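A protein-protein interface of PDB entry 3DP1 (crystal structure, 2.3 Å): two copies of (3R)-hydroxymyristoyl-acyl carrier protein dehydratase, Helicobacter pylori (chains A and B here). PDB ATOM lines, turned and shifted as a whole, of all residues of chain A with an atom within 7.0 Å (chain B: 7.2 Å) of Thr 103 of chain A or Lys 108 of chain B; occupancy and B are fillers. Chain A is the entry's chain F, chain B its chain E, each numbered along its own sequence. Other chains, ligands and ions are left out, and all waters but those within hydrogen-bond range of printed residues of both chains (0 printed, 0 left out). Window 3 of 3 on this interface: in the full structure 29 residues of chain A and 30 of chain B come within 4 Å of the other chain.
The backbone NH of Lys 106 of chain B is in hydrogen-bond range of the side-chain carboxylate of Asp 105 of chain A (2.8 Å). OD2 of Asp 105 of chain B sits close to OD1 of Asp 105 of chain A (3.1 Å). N of Phe 109 of chain B sits at hydrogen-bond distance from O of Met 102 of chain A (2.9 Å). O of Ile 104 of chain A lies within hydrogen-bond range of N of Val 107 of chain B (2.8 Å).
Thr 103 of chain A touches just these residues of chain B: Val 107 and Lys 108. Lys 108 of chain B touches just these residues of chain A: Met 102 (3.4 Å) and Thr 103 (3.5 Å). Printed residues of chain A within 4 Å of Val 107 of chain B: Thr 103 and Ile 104. Printed residues of chain B within 4 Å of Phe 101 of chain A: Phe 109. Printed residues of chain B within 4 Å of Met 102 of chain A: Lys 108 and Phe 109. Of the printed residues of chain B, Asp 105 of chain A touches Asp 105 and Lys 106. Tyr 100 of chain A touches none of the printed residues of chain B. The nearest residue of chain B that does not touch Thr 103 of chain A is Phe 109 of chain B (4.4 Å). The nearest residue of chain A that does not touch Lys 108 of chain B is Lys 152 of chain A (4.6 Å).
Printed residues of chain A that touch a printed residue of chain B: Phe 101, Met 102, Thr 103, Ile 104 and Asp 105. Hydrophobic or aromatic side chains of chain A within 4 Å of the printed part of chain B: Phe 101 and Ile 104. Of the 14 printed residues of chain B, 5 touch a printed residue of chain A. Hydrophobic or aromatic side chains of chain B that line the printed part of chain A: Val 107 and Phe 109. Among the printed residues, 10 pairs touch across the chains. Among the printed residues, no Asp or Glu carboxylate lies within 4 Å of a Lys or Arg side-chain nitrogen of the other chain.
Asp 105 of chain B touches its own counterpart, Asp 105 of chain A. Positions printed for both chains: 105 and 150.
Phe 101 of chain A touches Phe 109 of chain B (O to CD1, 3.4 Å). Lys 108 of chain B touches Met 102 of chain A (CA to O, 3.4 Å). Thr 103 of chain A touches Val 107 of chain B. CG2 of Thr 103 of chain A touches NZ of Lys 108 of chain B, 3.5 Å away. Ile 104 of chain A touches Lys 106 of chain B (O to N, 3.6 Å). Ile 104 of chain A touches Phe 109 of chain B.
N of Asp 105 of chain A lies within hydrogen-bond range of O of Glu 150 of chain A (3.0 Å). O of Lys 108 of chain B lies within hydrogen-bond range of N of Glu 148 of chain B. The backbone carbonyl oxygen of Lys 152 of chain A is in hydrogen-bond range of the backbone NH of Met 102 of chain A (2.8 Å). The backbone carbonyl oxygen (O) of Thr 103 of chain A lies within hydrogen-bond range of the backbone NH (N) of Lys 152 of chain A, 3.0 Å away. N of Asp 105 of chain B lies within hydrogen-bond range of O of Glu 150 of chain B, at 2.8 Å.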
ATOM      1  N   TYR A 100      -9.859 -25.294 -24.456  1.00  0.00           N
ATOM      2  CA  TYR A 100      -9.619 -23.859 -24.457  1.00  0.00           C
ATOM      3  C   TYR A 100      -8.188 -23.563 -24.045  1.00  0.00           C
ATOM      4  O   TYR A 100      -7.625 -24.225 -23.175  1.00  0.00           O
ATOM      5  CB  TYR A 100     -10.537 -23.139 -23.470  1.00  0.00           C
ATOM      6  CG  TYR A 100     -11.992 -23.081 -23.847  1.00  0.00           C
ATOM      7  CD1 TYR A 100     -12.913 -23.956 -23.275  1.00  0.00           C
ATOM      8  CD2 TYR A 100     -12.462 -22.114 -24.738  1.00  0.00           C
ATOM      9  CE1 TYR A 100     -14.267 -23.870 -23.576  1.00  0.00           C
ATOM     10  CE2 TYR A 100     -13.814 -22.017 -25.050  1.00  0.00           C
ATOM     11  CZ  TYR A 100     -14.715 -22.896 -24.464  1.00  0.00           C
ATOM     12  OH  TYR A 100     -16.067 -22.791 -24.742  1.00  0.00           O
ATOM     13  N   PHE A 101      -7.615 -22.554 -24.679  1.00  0.00           N
ATOM     14  CA  PHE A 101      -6.273 -22.108 -24.352  1.00  0.00           C
ATOM     15  C   PHE A 101      -6.465 -21.227 -23.120  1.00  0.00           C
ATOM     16  O   PHE A 101      -7.361 -20.382 -23.105  1.00  0.00           O
ATOM     17  CB  PHE A 101      -5.718 -21.264 -25.499  1.00  0.00           C
ATOM     18  CG  PHE A 101      -4.441 -21.788 -26.076  1.00  0.00           C
ATOM     19  CD1 PHE A 101      -3.260 -21.741 -25.347  1.00  0.00           C
ATOM     20  CD2 PHE A 101      -4.415 -22.319 -27.362  1.00  0.00           C
ATOM     21  CE1 PHE A 101      -2.069 -22.212 -25.893  1.00  0.00           C
ATOM     22  CE2 PHE A 101      -3.233 -22.790 -27.912  1.00  0.00           C
ATOM     23  CZ  PHE A 101      -2.059 -22.736 -27.178  1.00  0.00           C
ATOM     24  N   MET A 102      -5.655 -21.428 -22.088  1.00  0.00           N
ATOM     25  CA  MET A 102      -5.757 -20.609 -20.875  1.00  0.00           C
ATOM     26  C   MET A 102      -4.584 -19.623 -20.774  1.00  0.00           C
ATOM     27  O   MET A 102      -4.785 -18.431 -20.518  1.00  0.00           O
ATOM     28  CB  MET A 102      -5.790 -21.498 -19.626  1.00  0.00           C
ATOM     29  CG  MET A 102      -7.064 -22.315 -19.478  1.00  0.00           C
ATOM     30  SD  MET A 102      -7.047 -23.252 -17.940  1.00  0.00           S
ATOM     31  CE  MET A 102      -7.254 -21.925 -16.730  1.00  0.00           C
ATOM     32  N   THR A 103      -3.366 -20.130 -20.963  1.00  0.00           N
ATOM     33  CA  THR A 103      -2.166 -19.297 -20.914  1.00  0.00           C
ATOM     34  C   THR A 103      -1.080 -19.816 -21.842  1.00  0.00           C
ATOM     35  O   THR A 103      -1.045 -20.995 -22.196  1.00  0.00           O
ATOM     36  CB  THR A 103      -1.543 -19.223 -19.491  1.00  0.00           C
ATOM     37  OG1 THR A 103      -1.066 -20.521 -19.101  1.00  0.00           O
ATOM     38  CG2 THR A 103      -2.569 -18.709 -18.477  1.00  0.00           C
ATOM     39  N   ILE A 104      -0.190 -18.909 -22.226  1.00  0.00           N
ATOM     40  CA  ILE A 104       0.940 -19.223 -23.087  1.00  0.00           C
ATOM     41  C   ILE A 104       2.097 -18.414 -22.520  1.00  0.00           C
ATOM     42  O   ILE A 104       1.922 -17.251 -22.158  1.00  0.00           O
ATOM     43  CB  ILE A 104       0.710 -18.756 -24.536  1.00  0.00           C
ATOM     44  CG1 ILE A 104      -0.575 -19.368 -25.097  1.00  0.00           C
ATOM     45  CG2 ILE A 104       1.898 -19.143 -25.387  1.00  0.00           C
ATOM     46  CD1 ILE A 104      -0.946 -18.835 -26.472  1.00  0.00           C
ATOM     47  N   ASP A 105       3.277 -19.017 -22.437  1.00  0.00           N
ATOM     48  CA  ASP A 105       4.409 -18.276 -21.900  1.00  0.00           C
ATOM     49  C   ASP A 105       5.760 -18.855 -22.299  1.00  0.00           C
ATOM     50  O   ASP A 105       5.865 -20.012 -22.719  1.00  0.00           O
ATOM     51  CB  ASP A 105       4.291 -18.187 -20.369  1.00  0.00           C
ATOM     52  CG  ASP A 105       5.188 -17.104 -19.770  1.00  0.00           C
ATOM     53  OD1 ASP A 105       5.489 -16.113 -20.478  1.00  0.00           O
ATOM     54  OD2 ASP A 105       5.576 -17.235 -18.587  1.00  0.00           O
ATOM     55  N   TRP A 133      -4.568 -28.519 -17.754  1.00  0.00           N
ATOM     56  CA  TRP A 133      -3.234 -29.042 -18.044  1.00  0.00           C
ATOM     57  C   TRP A 133      -2.185 -28.025 -18.485  1.00  0.00           C
ATOM     58  O   TRP A 133      -2.401 -27.241 -19.413  1.00  0.00           O
ATOM     59  CB  TRP A 133      -3.332 -30.145 -19.093  1.00  0.00           C
ATOM     60  CG  TRP A 133      -3.948 -31.385 -18.563  1.00  0.00           C
ATOM     61  CD1 TRP A 133      -5.237 -31.544 -18.131  1.00  0.00           C
ATOM     62  CD2 TRP A 133      -3.295 -32.643 -18.348  1.00  0.00           C
ATOM     63  NE1 TRP A 133      -5.421 -32.819 -17.656  1.00  0.00           N
ATOM     64  CE2 TRP A 133      -4.247 -33.515 -17.775  1.00  0.00           C
ATOM     65  CE3 TRP A 133      -1.997 -33.116 -18.581  1.00  0.00           C
ATOM     66  CZ2 TRP A 133      -3.940 -34.834 -17.429  1.00  0.00           C
ATOM     67  CZ3 TRP A 133      -1.691 -34.429 -18.237  1.00  0.00           C
ATOM     68  CH2 TRP A 133      -2.661 -35.272 -17.667  1.00  0.00           C
ATOM     69  N   GLN A 134      -1.042 -28.054 -17.809  1.00  0.00           N
ATOM     70  CA  GLN A 134       0.060 -27.157 -18.122  1.00  0.00           C
ATOM     71  C   GLN A 134       1.221 -27.992 -18.651  1.00  0.00           C
ATOM     72  O   GLN A 134       1.812 -28.783 -17.915  1.00  0.00           O
ATOM     73  CB  GLN A 134       0.505 -26.389 -16.873  1.00  0.00           C
ATOM     74  CG  GLN A 134       1.700 -25.469 -17.113  1.00  0.00           C
ATOM     75  CD  GLN A 134       2.222 -24.804 -15.837  1.00  0.00           C
ATOM     76  OE1 GLN A 134       3.302 -24.196 -15.833  1.00  0.00           O
ATOM     77  NE2 GLN A 134       1.456 -24.913 -14.750  1.00  0.00           N
ATOM     78  N   GLU A 150       5.532 -22.960 -23.441  1.00  0.00           N
ATOM     79  CA  GLU A 150       4.864 -23.489 -22.268  1.00  0.00           C
ATOM     80  C   GLU A 150       3.443 -23.016 -22.450  1.00  0.00           C
ATOM     81  O   GLU A 150       3.212 -21.921 -22.959  1.00  0.00           O
ATOM     82  CB  GLU A 150       5.446 -22.904 -20.982  1.00  0.00           C
ATOM     83  CG  GLU A 150       6.593 -23.711 -20.407  1.00  0.00           C
ATOM     84  CD  GLU A 150       7.195 -23.064 -19.176  1.00  0.00           C
ATOM     85  OE1 GLU A 150       6.427 -22.558 -18.328  1.00  0.00           O
ATOM     86  OE2 GLU A 150       8.437 -23.070 -19.053  1.00  0.00           O
ATOM     87  N   LEU A 151       2.489 -23.838 -22.044  1.00  0.00           N
ATOM     88  CA  LEU A 151       1.100 -23.467 -22.205  1.00  0.00           C
ATOM     89  C   LEU A 151       0.212 -24.259 -21.266  1.00  0.00           C
ATOM     90  O   LEU A 151       0.558 -25.364 -20.844  1.00  0.00           O
ATOM     91  CB  LEU A 151       0.676 -23.694 -23.661  1.00  0.00           C
ATOM     92  CG  LEU A 151       0.709 -25.143 -24.156  1.00  0.00           C
ATOM     93  CD1 LEU A 151      -0.652 -25.791 -23.918  1.00  0.00           C
ATOM     94  CD2 LEU A 151       1.055 -25.186 -25.634  1.00  0.00           C
ATOM     95  N   LYS A 152      -0.927 -23.665 -20.928  1.00  0.00           N
ATOM     96  CA  LYS A 152      -1.899 -24.295 -20.059  1.00  0.00           C
ATOM     97  C   LYS A 152      -3.244 -24.224 -20.773  1.00  0.00           C
ATOM     98  O   LYS A 152      -3.658 -23.155 -21.238  1.00  0.00           O
ATOM     99  CB  LYS A 152      -1.971 -23.569 -18.719  1.00  0.00           C
ATOM    100  CG  LYS A 152      -2.800 -24.302 -17.678  1.00  0.00           C
ATOM    101  CD  LYS A 152      -2.779 -23.592 -16.335  1.00  0.00           C
ATOM    102  CE  LYS A 152      -3.525 -22.269 -16.391  1.00  0.00           C
ATOM    103  NZ  LYS A 152      -3.405 -21.529 -15.108  1.00  0.00           N
ATOM    104  N   ALA A 153      -3.910 -25.370 -20.877  1.00  0.00           N
ATOM    105  CA  ALA A 153      -5.199 -25.442 -21.547  1.00  0.00           C
ATOM    106  C   ALA A 153      -6.218 -26.154 -20.671  1.00  0.00           C
ATOM    107  O   ALA A 153      -5.859 -26.868 -19.738  1.00  0.00           O
ATOM    108  CB  ALA A 153      -5.052 -26.170 -22.879  1.00  0.00           C
ATOM    109  N   VAL B  71      -3.600 -13.563 -30.629  1.00  0.00           N
ATOM    110  CA  VAL B  71      -2.224 -13.148 -30.400  1.00  0.00           C
ATOM    111  C   VAL B  71      -1.638 -12.639 -31.712  1.00  0.00           C
ATOM    112  O   VAL B  71      -0.945 -11.622 -31.742  1.00  0.00           O
ATOM    113  CB  VAL B  71      -1.368 -14.321 -29.883  1.00  0.00           C
ATOM    114  CG1 VAL B  71       0.098 -13.904 -29.777  1.00  0.00           C
ATOM    115  CG2 VAL B  71      -1.883 -14.759 -28.537  1.00  0.00           C
ATOM    116  N   ASP B 105       5.069 -13.971 -24.474  1.00  0.00           N
ATOM    117  CA  ASP B 105       5.059 -14.224 -23.035  1.00  0.00           C
ATOM    118  C   ASP B 105       3.800 -13.700 -22.350  1.00  0.00           C
ATOM    119  O   ASP B 105       3.057 -12.892 -22.914  1.00  0.00           O
ATOM    120  CB  ASP B 105       6.272 -13.575 -22.361  1.00  0.00           C
ATOM    121  CG  ASP B 105       7.576 -14.198 -22.778  1.00  0.00           C
ATOM    122  OD1 ASP B 105       8.240 -13.650 -23.690  1.00  0.00           O
ATOM    123  OD2 ASP B 105       7.939 -15.244 -22.193  1.00  0.00           O
ATOM    124  N   LYS B 106       3.576 -14.167 -21.126  1.00  0.00           N
ATOM    125  CA  LYS B 106       2.434 -13.734 -20.328  1.00  0.00           C
ATOM    126  C   LYS B 106       1.107 -13.657 -21.077  1.00  0.00           C
ATOM    127  O   LYS B 106       0.390 -12.664 -20.968  1.00  0.00           O
ATOM    128  CB  LYS B 106       2.712 -12.359 -19.702  1.00  0.00           C
ATOM    129  CG  LYS B 106       3.693 -12.353 -18.538  1.00  0.00           C
ATOM    130  CD  LYS B 106       5.125 -12.529 -18.998  1.00  0.00           C
ATOM    131  CE  LYS B 106       6.111 -12.206 -17.871  1.00  0.00           C
ATOM    132  NZ  LYS B 106       7.510 -12.276 -18.383  1.00  0.00           N
ATOM    133  N   VAL B 107       0.782 -14.682 -21.849  1.00  0.00           N
ATOM    134  CA  VAL B 107      -0.488 -14.678 -22.561  1.00  0.00           C
ATOM    135  C   VAL B 107      -1.530 -15.323 -21.656  1.00  0.00           C
ATOM    136  O   VAL B 107      -1.284 -16.367 -21.054  1.00  0.00           O
ATOM    137  CB  VAL B 107      -0.404 -15.461 -23.881  1.00  0.00           C
ATOM    138  CG1 VAL B 107      -1.781 -15.535 -24.526  1.00  0.00           C
ATOM    139  CG2 VAL B 107       0.574 -14.779 -24.822  1.00  0.00           C
ATOM    140  N   LYS B 108      -2.687 -14.688 -21.547  1.00  0.00           N
ATOM    141  CA  LYS B 108      -3.758 -15.213 -20.709  1.00  0.00           C
ATOM    142  C   LYS B 108      -5.055 -14.936 -21.449  1.00  0.00           C
ATOM    143  O   LYS B 108      -5.296 -13.810 -21.880  1.00  0.00           O
ATOM    144  CB  LYS B 108      -3.757 -14.502 -19.344  1.00  0.00           C
ATOM    145  CG  LYS B 108      -4.167 -15.357 -18.140  1.00  0.00           C
ATOM    146  CD  LYS B 108      -5.677 -15.586 -18.064  1.00  0.00           C
ATOM    147  CE  LYS B 108      -6.074 -16.493 -16.875  1.00  0.00           C
ATOM    148  NZ  LYS B 108      -5.642 -17.937 -17.029  1.00  0.00           N
ATOM    149  N   PHE B 109      -5.866 -15.972 -21.632  1.00  0.00           N
ATOM    150  CA  PHE B 109      -7.147 -15.820 -22.309  1.00  0.00           C
ATOM    151  C   PHE B 109      -8.199 -15.888 -21.207  1.00  0.00           C
ATOM    152  O   PHE B 109      -8.198 -16.809 -20.398  1.00  0.00           O
ATOM    153  CB  PHE B 109      -7.345 -16.943 -23.342  1.00  0.00           C
ATOM    154  CG  PHE B 109      -6.249 -17.019 -24.373  1.00  0.00           C
ATOM    155  CD1 PHE B 109      -5.257 -17.993 -24.289  1.00  0.00           C
ATOM    156  CD2 PHE B 109      -6.201 -16.103 -25.423  1.00  0.00           C
ATOM    157  CE1 PHE B 109      -4.229 -18.055 -25.240  1.00  0.00           C
ATOM    158  CE2 PHE B 109      -5.183 -16.154 -26.377  1.00  0.00           C
ATOM    159  CZ  PHE B 109      -4.197 -17.128 -26.288  1.00  0.00           C
ATOM    160  N   ARG B 110      -9.094 -14.913 -21.164  1.00  0.00           N
ATOM    161  CA  ARG B 110     -10.099 -14.886 -20.104  1.00  0.00           C
ATOM    162  C   ARG B 110     -11.526 -15.148 -20.577  1.00  0.00           C
ATOM    163  O   ARG B 110     -12.317 -15.754 -19.857  1.00  0.00           O
ATOM    164  CB  ARG B 110     -10.036 -13.535 -19.380  1.00  0.00           C
ATOM    165  CG  ARG B 110      -8.613 -13.052 -19.097  1.00  0.00           C
ATOM    166  CD  ARG B 110      -8.590 -11.738 -18.304  1.00  0.00           C
ATOM    167  NE  ARG B 110      -8.810 -11.972 -16.881  1.00  0.00           N
ATOM    168  CZ  ARG B 110      -7.858 -11.910 -15.953  1.00  0.00           C
ATOM    169  NH1 ARG B 110      -6.608 -11.608 -16.284  1.00  0.00           N
ATOM    170  NH2 ARG B 110      -8.158 -12.183 -14.691  1.00  0.00           N
ATOM    171  N   ILE B 111     -11.843 -14.696 -21.789  1.00  0.00           N
ATOM    172  CA  ILE B 111     -13.181 -14.844 -22.354  1.00  0.00           C
ATOM    173  C   ILE B 111     -13.092 -15.278 -23.811  1.00  0.00           C
ATOM    174  O   ILE B 111     -12.317 -14.722 -24.577  1.00  0.00           O
ATOM    175  CB  ILE B 111     -13.947 -13.501 -22.292  1.00  0.00           C
ATOM    176  CG1 ILE B 111     -14.020 -13.010 -20.845  1.00  0.00           C
ATOM    177  CG2 ILE B 111     -15.338 -13.656 -22.884  1.00  0.00           C
ATOM    178  CD1 ILE B 111     -14.572 -11.609 -20.705  1.00  0.00           C
ATOM    179  N   VAL B 145     -11.710  -7.102 -21.077  1.00  0.00           N
ATOM    180  CA  VAL B 145     -10.471  -7.751 -21.480  1.00  0.00           C
ATOM    181  C   VAL B 145     -10.748  -9.217 -21.741  1.00  0.00           C
ATOM    182  O   VAL B 145     -11.183  -9.962 -20.861  1.00  0.00           O
ATOM    183  CB  VAL B 145      -9.376  -7.624 -20.402  1.00  0.00           C
ATOM    184  CG1 VAL B 145      -8.177  -8.471 -20.782  1.00  0.00           C
ATOM    185  CG2 VAL B 145      -8.960  -6.172 -20.259  1.00  0.00           C
ATOM    186  N   VAL B 146     -10.468  -9.630 -22.965  1.00  0.00           N
ATOM    187  CA  VAL B 146     -10.722 -10.992 -23.381  1.00  0.00           C
ATOM    188  C   VAL B 146      -9.411 -11.775 -23.401  1.00  0.00           C
ATOM    189  O   VAL B 146      -9.391 -13.002 -23.280  1.00  0.00           O
ATOM    190  CB  VAL B 146     -11.413 -10.956 -24.770  1.00  0.00           C
ATOM    191  CG1 VAL B 146     -10.443 -11.316 -25.875  1.00  0.00           C
ATOM    192  CG2 VAL B 146     -12.635 -11.819 -24.753  1.00  0.00           C
ATOM    193  N   ALA B 147      -8.316 -11.042 -23.528  1.00  0.00           N
ATOM    194  CA  ALA B 147      -6.998 -11.652 -23.558  1.00  0.00           C
ATOM    195  C   ALA B 147      -5.920 -10.619 -23.280  1.00  0.00           C
ATOM    196  O   ALA B 147      -6.121  -9.416 -23.467  1.00  0.00           O
ATOM    197  CB  ALA B 147      -6.751 -12.306 -24.916  1.00  0.00           C
ATOM    198  N   GLU B 148      -4.781 -11.098 -22.812  1.00  0.00           N
ATOM    199  CA  GLU B 148      -3.656 -10.231 -22.542  1.00  0.00           C
ATOM    200  C   GLU B 148      -2.416 -10.941 -23.061  1.00  0.00           C
ATOM    201  O   GLU B 148      -2.322 -12.174 -23.004  1.00  0.00           O
ATOM    202  CB  GLU B 148      -3.555  -9.915 -21.043  1.00  0.00           C
ATOM    203  CG  GLU B 148      -3.692 -11.103 -20.119  1.00  0.00           C
ATOM    204  CD  GLU B 148      -3.810 -10.686 -18.662  1.00  0.00           C
ATOM    205  OE1 GLU B 148      -4.854 -10.124 -18.274  1.00  0.00           O
ATOM    206  OE2 GLU B 148      -2.847 -10.917 -17.905  1.00  0.00           O
ATOM    207  N   ALA B 149      -1.486 -10.171 -23.614  1.00  0.00           N
ATOM    208  CA  ALA B 149      -0.275 -10.755 -24.155  1.00  0.00           C
ATOM    209  C   ALA B 149       0.893  -9.788 -24.242  1.00  0.00           C
ATOM    210  O   ALA B 149       0.744  -8.563 -24.194  1.00  0.00           O
ATOM    211  CB  ALA B 149      -0.555 -11.340 -25.531  1.00  0.00           C
ATOM    212  N   GLU B 150       2.068 -10.375 -24.382  1.00  0.00           N
ATOM    213  CA  GLU B 150       3.297  -9.628 -24.500  1.00  0.00           C
ATOM    214  C   GLU B 150       4.080 -10.347 -25.590  1.00  0.00           C
ATOM    215  O   GLU B 150       4.167 -11.575 -25.582  1.00  0.00           O
ATOM    216  CB  GLU B 150       4.022  -9.669 -23.158  1.00  0.00           C
ATOM    217  CG  GLU B 150       5.444  -9.193 -23.171  1.00  0.00           C
ATOM    218  CD  GLU B 150       6.013  -9.138 -21.765  1.00  0.00           C
ATOM    219  OE1 GLU B 150       7.236  -9.347 -21.612  1.00  0.00           O
ATOM    220  OE2 GLU B 150       5.237  -8.878 -20.817  1.00  0.00           O
